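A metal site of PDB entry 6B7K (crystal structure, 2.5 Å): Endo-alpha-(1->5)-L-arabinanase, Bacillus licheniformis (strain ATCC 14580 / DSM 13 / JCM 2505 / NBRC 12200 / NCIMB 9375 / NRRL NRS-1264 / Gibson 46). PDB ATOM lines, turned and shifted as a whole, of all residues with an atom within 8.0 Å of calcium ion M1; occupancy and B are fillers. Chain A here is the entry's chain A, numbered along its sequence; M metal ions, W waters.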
ATOM      1  N   PRO A  24       8.492 -18.869 -29.528  1.00  0.00           N
ATOM      2  CA  PRO A  24       7.441 -18.752 -28.506  1.00  0.00           C
ATOM      3  C   PRO A  24       7.547 -19.802 -27.413  1.00  0.00           C
ATOM      4  O   PRO A  24       8.144 -20.869 -27.570  1.00  0.00           O
ATOM      5  CB  PRO A  24       6.163 -18.957 -29.329  1.00  0.00           C
ATOM      6  CG  PRO A  24       6.568 -19.931 -30.361  1.00  0.00           C
ATOM      7  CD  PRO A  24       8.000 -19.599 -30.717  1.00  0.00           C
ATOM      8  N   SER A  25       6.932 -19.459 -26.280  1.00  0.00           N
ATOM      9  CA  SER A  25       6.752 -20.390 -25.163  1.00  0.00           C
ATOM     10  C   SER A  25       5.396 -20.092 -24.545  1.00  0.00           C
ATOM     11  O   SER A  25       5.142 -18.959 -24.117  1.00  0.00           O
ATOM     12  CB  SER A  25       7.867 -20.243 -24.128  1.00  0.00           C
ATOM     13  OG  SER A  25       7.729 -21.193 -23.075  1.00  0.00           O
ATOM     14  N   ILE A  26       4.524 -21.102 -24.504  1.00  0.00           N
ATOM     15  CA  ILE A  26       3.135 -20.906 -24.101  1.00  0.00           C
ATOM     16  C   ILE A  26       2.974 -21.182 -22.624  1.00  0.00           C
ATOM     17  O   ILE A  26       3.645 -22.038 -22.032  1.00  0.00           O
ATOM     18  CB  ILE A  26       2.192 -21.802 -24.941  1.00  0.00           C
ATOM     19  CG1 ILE A  26       0.724 -21.442 -24.682  1.00  0.00           C
ATOM     20  CG2 ILE A  26       2.436 -23.268 -24.655  1.00  0.00           C
ATOM     21  CD1 ILE A  26       0.363 -20.020 -25.022  1.00  0.00           C
ATOM     22  N   PRO A  83      12.268 -16.674 -24.828  1.00  0.00           N
ATOM     23  CA  PRO A  83      11.883 -16.820 -23.424  1.00  0.00           C
ATOM     24  C   PRO A  83      11.234 -18.172 -23.157  1.00  0.00           C
ATOM     25  O   PRO A  83      10.718 -18.835 -24.057  1.00  0.00           O
ATOM     26  CB  PRO A  83      10.887 -15.687 -23.207  1.00  0.00           C
ATOM     27  CG  PRO A  83      10.252 -15.508 -24.541  1.00  0.00           C
ATOM     28  CD  PRO A  83      11.316 -15.821 -25.566  1.00  0.00           C
ATOM     29  N   ASP A  84      11.312 -18.581 -21.888  1.00  0.00           N
ATOM     30  CA  ASP A  84      10.639 -19.790 -21.421  1.00  0.00           C
ATOM     31  C   ASP A  84       9.868 -19.463 -20.157  1.00  0.00           C
ATOM     32  O   ASP A  84      10.448 -18.943 -19.191  1.00  0.00           O
ATOM     33  CB  ASP A  84      11.627 -20.925 -21.158  1.00  0.00           C
ATOM     34  CG  ASP A  84      10.949 -22.185 -20.674  1.00  0.00           C
ATOM     35  OD1 ASP A  84      10.037 -22.673 -21.377  1.00  0.00           O
ATOM     36  OD2 ASP A  84      11.321 -22.694 -19.592  1.00  0.00           O
ATOM     37  N   ILE A  85       8.579 -19.761 -20.156  1.00  0.00           N
ATOM     38  CA  ILE A  85       7.685 -19.424 -19.052  1.00  0.00           C
ATOM     39  C   ILE A  85       7.070 -20.714 -18.504  1.00  0.00           C
ATOM     40  O   ILE A  85       6.650 -21.586 -19.263  1.00  0.00           O
ATOM     41  CB  ILE A  85       6.588 -18.440 -19.499  1.00  0.00           C
ATOM     42  CG1 ILE A  85       5.658 -18.091 -18.336  1.00  0.00           C
ATOM     43  CG2 ILE A  85       5.830 -18.989 -20.695  1.00  0.00           C
ATOM     44  CD1 ILE A  85       6.345 -17.363 -17.199  1.00  0.00           C
ATOM     45  N   SER A  86       7.039 -20.822 -17.178  1.00  0.00           N
ATOM     46  CA  SER A  86       6.425 -21.974 -16.528  1.00  0.00           C
ATOM     47  C   SER A  86       6.171 -21.634 -15.065  1.00  0.00           C
ATOM     48  O   SER A  86       6.800 -20.735 -14.506  1.00  0.00           O
ATOM     49  CB  SER A  86       7.302 -23.219 -16.647  1.00  0.00           C
ATOM     50  OG  SER A  86       8.607 -22.973 -16.141  1.00  0.00           O
ATOM     51  N   PRO A 141      16.788 -21.150 -23.562  1.00  0.00           N
ATOM     52  CA  PRO A 141      16.627 -21.933 -22.335  1.00  0.00           C
ATOM     53  C   PRO A 141      15.262 -22.587 -22.262  1.00  0.00           C
ATOM     54  O   PRO A 141      14.321 -22.225 -22.977  1.00  0.00           O
ATOM     55  CB  PRO A 141      16.800 -20.893 -21.232  1.00  0.00           C
ATOM     56  CG  PRO A 141      16.247 -19.660 -21.837  1.00  0.00           C
ATOM     57  CD  PRO A 141      16.570 -19.716 -23.315  1.00  0.00           C
ATOM     58  N   ASP A 142      15.158 -23.574 -21.372  1.00  0.00           N
ATOM     59  CA  ASP A 142      13.898 -24.280 -21.183  1.00  0.00           C
ATOM     60  C   ASP A 142      13.957 -25.049 -19.870  1.00  0.00           C
ATOM     61  O   ASP A 142      14.873 -25.861 -19.668  1.00  0.00           O
ATOM     62  CB  ASP A 142      13.639 -25.240 -22.341  1.00  0.00           C
ATOM     63  CG  ASP A 142      12.199 -25.717 -22.386  1.00  0.00           C
ATOM     64  OD1 ASP A 142      11.337 -24.941 -22.843  1.00  0.00           O
ATOM     65  OD2 ASP A 142      11.941 -26.849 -21.940  1.00  0.00           O
ATOM     66  N   LEU A 143      13.001 -24.785 -18.990  1.00  0.00           N
ATOM     67  CA  LEU A 143      12.907 -25.460 -17.707  1.00  0.00           C
ATOM     68  C   LEU A 143      12.095 -26.745 -17.842  1.00  0.00           C
ATOM     69  O   LEU A 143      11.112 -26.798 -18.585  1.00  0.00           O
ATOM     70  CB  LEU A 143      12.261 -24.528 -16.677  1.00  0.00           C
ATOM     71  CG  LEU A 143      11.955 -25.050 -15.274  1.00  0.00           C
ATOM     72  CD1 LEU A 143      13.224 -25.457 -14.550  1.00  0.00           C
ATOM     73  CD2 LEU A 143      11.200 -24.004 -14.476  1.00  0.00           C
ATOM     74  N   VAL A 144      12.520 -27.781 -17.117  1.00  0.00           N
ATOM     75  CA  VAL A 144      11.835 -29.067 -17.114  1.00  0.00           C
ATOM     76  C   VAL A 144      11.950 -29.655 -15.710  1.00  0.00           C
ATOM     77  O   VAL A 144      12.983 -29.534 -15.048  1.00  0.00           O
ATOM     78  CB  VAL A 144      12.412 -30.018 -18.177  1.00  0.00           C
ATOM     79  CG1 VAL A 144      13.919 -30.138 -18.038  1.00  0.00           C
ATOM     80  CG2 VAL A 144      11.750 -31.389 -18.089  1.00  0.00           C
ATOM     81  N   SER A 154      17.569 -27.100 -19.967  1.00  0.00           N
ATOM     82  CA  SER A 154      18.189 -27.448 -21.236  1.00  0.00           C
ATOM     83  C   SER A 154      18.312 -26.194 -22.099  1.00  0.00           C
ATOM     84  O   SER A 154      17.398 -25.367 -22.130  1.00  0.00           O
ATOM     85  CB  SER A 154      17.383 -28.514 -21.975  1.00  0.00           C
ATOM     86  OG  SER A 154      16.117 -28.008 -22.363  1.00  0.00           O
ATOM     87  N   PRO A 194      15.849 -26.284 -27.534  1.00  0.00           N
ATOM     88  CA  PRO A 194      15.420 -27.556 -26.940  1.00  0.00           C
ATOM     89  C   PRO A 194      14.342 -27.354 -25.894  1.00  0.00           C
ATOM     90  O   PRO A 194      14.301 -26.349 -25.184  1.00  0.00           O
ATOM     91  CB  PRO A 194      16.708 -28.075 -26.307  1.00  0.00           C
ATOM     92  CG  PRO A 194      17.402 -26.826 -25.865  1.00  0.00           C
ATOM     93  CD  PRO A 194      17.057 -25.757 -26.879  1.00  0.00           C
ATOM     94  N   ASN A 195      13.455 -28.342 -25.801  1.00  0.00           N
ATOM     95  CA  ASN A 195      12.514 -28.413 -24.684  1.00  0.00           C
ATOM     96  C   ASN A 195      12.264 -29.875 -24.351  1.00  0.00           C
ATOM     97  O   ASN A 195      12.085 -30.691 -25.255  1.00  0.00           O
ATOM     98  CB  ASN A 195      11.198 -27.664 -24.997  1.00  0.00           C
ATOM     99  CG  ASN A 195      10.396 -28.328 -26.088  1.00  0.00           C
ATOM    100  OD1 ASN A 195      10.522 -28.003 -27.267  1.00  0.00           O
ATOM    101  ND2 ASN A 195       9.528 -29.252 -25.694  1.00  0.00           N
ATOM    102  N   ILE A 196      12.282 -30.193 -23.063  1.00  0.00           N
ATOM    103  CA  ILE A 196      12.183 -31.565 -22.580  1.00  0.00           C
ATOM    104  C   ILE A 196      10.903 -31.707 -21.761  1.00  0.00           C
ATOM    105  O   ILE A 196      10.530 -30.793 -21.018  1.00  0.00           O
ATOM    106  CB  ILE A 196      13.402 -31.951 -21.728  1.00  0.00           C
ATOM    107  CG1 ILE A 196      14.701 -31.532 -22.421  1.00  0.00           C
ATOM    108  CG2 ILE A 196      13.408 -33.448 -21.454  1.00  0.00           C
ATOM    109  CD1 ILE A 196      15.939 -31.842 -21.619  1.00  0.00           C
ATOM    110  N   THR A 197      10.236 -32.854 -21.902  1.00  0.00           N
ATOM    111  CA  THR A 197       9.050 -33.151 -21.121  1.00  0.00           C
ATOM    112  C   THR A 197       9.025 -34.625 -20.775  1.00  0.00           C
ATOM    113  O   THR A 197       9.500 -35.473 -21.543  1.00  0.00           O
ATOM    114  CB  THR A 197       7.757 -32.765 -21.864  1.00  0.00           C
ATOM    115  OG1 THR A 197       6.624 -33.172 -21.083  1.00  0.00           O
ATOM    116  CG2 THR A 197       7.711 -33.433 -23.227  1.00  0.00           C
ATOM    117  N   GLN A 263       9.942 -24.690 -30.977  1.00  0.00           N
ATOM    118  CA  GLN A 263       8.692 -25.170 -30.405  1.00  0.00           C
ATOM    119  C   GLN A 263       8.784 -25.212 -28.876  1.00  0.00           C
ATOM    120  O   GLN A 263       9.850 -25.017 -28.284  1.00  0.00           O
ATOM    121  CB  GLN A 263       8.362 -26.566 -30.944  1.00  0.00           C
ATOM    122  CG  GLN A 263       9.178 -27.676 -30.313  1.00  0.00           C
ATOM    123  CD  GLN A 263      10.684 -27.502 -30.519  1.00  0.00           C
ATOM    124  OE1 GLN A 263      11.127 -27.143 -31.605  1.00  0.00           O
ATOM    125  NE2 GLN A 263      11.456 -27.733 -29.464  1.00  0.00           N
ATOM    126  N   ASP A 264       7.634 -25.461 -28.260  1.00  0.00           N
ATOM    127  CA  ASP A 264       7.558 -25.729 -26.833  1.00  0.00           C
ATOM    128  C   ASP A 264       6.251 -26.452 -26.579  1.00  0.00           C
ATOM    129  O   ASP A 264       5.279 -26.274 -27.318  1.00  0.00           O
ATOM    130  CB  ASP A 264       7.654 -24.440 -26.007  1.00  0.00           C
ATOM    131  CG  ASP A 264       8.143 -24.693 -24.594  1.00  0.00           C
ATOM    132  OD1 ASP A 264       8.250 -25.868 -24.194  1.00  0.00           O
ATOM    133  OD2 ASP A 264       8.433 -23.708 -23.880  1.00  0.00           O
ATOM    134  N   VAL A 265       6.238 -27.273 -25.525  1.00  0.00           N
ATOM    135  CA  VAL A 265       5.077 -28.092 -25.192  1.00  0.00           C
ATOM    136  C   VAL A 265       4.547 -27.669 -23.820  1.00  0.00           C
ATOM    137  O   VAL A 265       5.327 -27.327 -22.919  1.00  0.00           O
ATOM    138  CB  VAL A 265       5.417 -29.597 -25.207  1.00  0.00           C
ATOM    139  CG1 VAL A 265       5.727 -30.060 -26.617  1.00  0.00           C
ATOM    140  CG2 VAL A 265       6.597 -29.894 -24.276  1.00  0.00           C
ATOM    141  N   LEU A 266       3.228 -27.682 -23.678  1.00  0.00           N
ATOM    142  CA  LEU A 266       2.569 -27.298 -22.435  1.00  0.00           C
ATOM    143  C   LEU A 266       1.631 -28.417 -22.001  1.00  0.00           C
ATOM    144  O   LEU A 266       0.771 -28.850 -22.768  1.00  0.00           O
ATOM    145  CB  LEU A 266       1.777 -25.997 -22.609  1.00  0.00           C
ATOM    146  CG  LEU A 266       0.823 -25.625 -21.461  1.00  0.00           C
ATOM    147  CD1 LEU A 266       1.595 -25.338 -20.187  1.00  0.00           C
ATOM    148  CD2 LEU A 266      -0.044 -24.440 -21.859  1.00  0.00           C
ATOM    149  N   VAL A 272       3.327 -25.458 -29.116  1.00  0.00           N
ATOM    150  CA  VAL A 272       3.344 -24.179 -29.785  1.00  0.00           C
ATOM    151  C   VAL A 272       4.610 -24.067 -30.621  1.00  0.00           C
ATOM    152  O   VAL A 272       5.561 -24.817 -30.435  1.00  0.00           O
ATOM    153  CB  VAL A 272       3.225 -22.999 -28.800  1.00  0.00           C
ATOM    154  CG1 VAL A 272       1.829 -22.949 -28.215  1.00  0.00           C
ATOM    155  CG2 VAL A 272       4.286 -23.120 -27.715  1.00  0.00           C
HETATM  156 CA    CA M   1       9.191 -24.919 -21.812  1.00  0.00          CA
HETATM  157 CA    CA M   2      12.346 -22.608 -25.662  1.00  0.00          CA
HETATM  158  O   HOH W   1       7.221 -26.560 -21.346  1.00  0.00           O
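The backbone carbonyl oxygen (O) of Ser 154 sits at hydrogen-bond distance from the backbone NH (N) of Asp 142. The side-chain hydroxyl of Ser 25 lies close to the side-chain carboxylate of Asp 84 (3.2 Å). OD2 of Asp 84 sits at hydrogen-bond distance from N of Leu 143, at 2.7 Å. The side-chain carboxylate of Asp 264 lies close to the side-chain hydroxyl of Ser 25 (2.7 Å). The backbone NH (N) of Val 272 is in hydrogen-bond range of the backbone carbonyl oxygen (O) of Asp 264 (2.8 Å).
The nearest printed residue that does not touch calcium ion M1 is Ser 25 (4.2 Å).
Calcium ion M1 is bound by OD1 of Asp 142, OD1 of Asp 84, OD2 of Asp 264, water W1 and OD1 of Asp 264.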
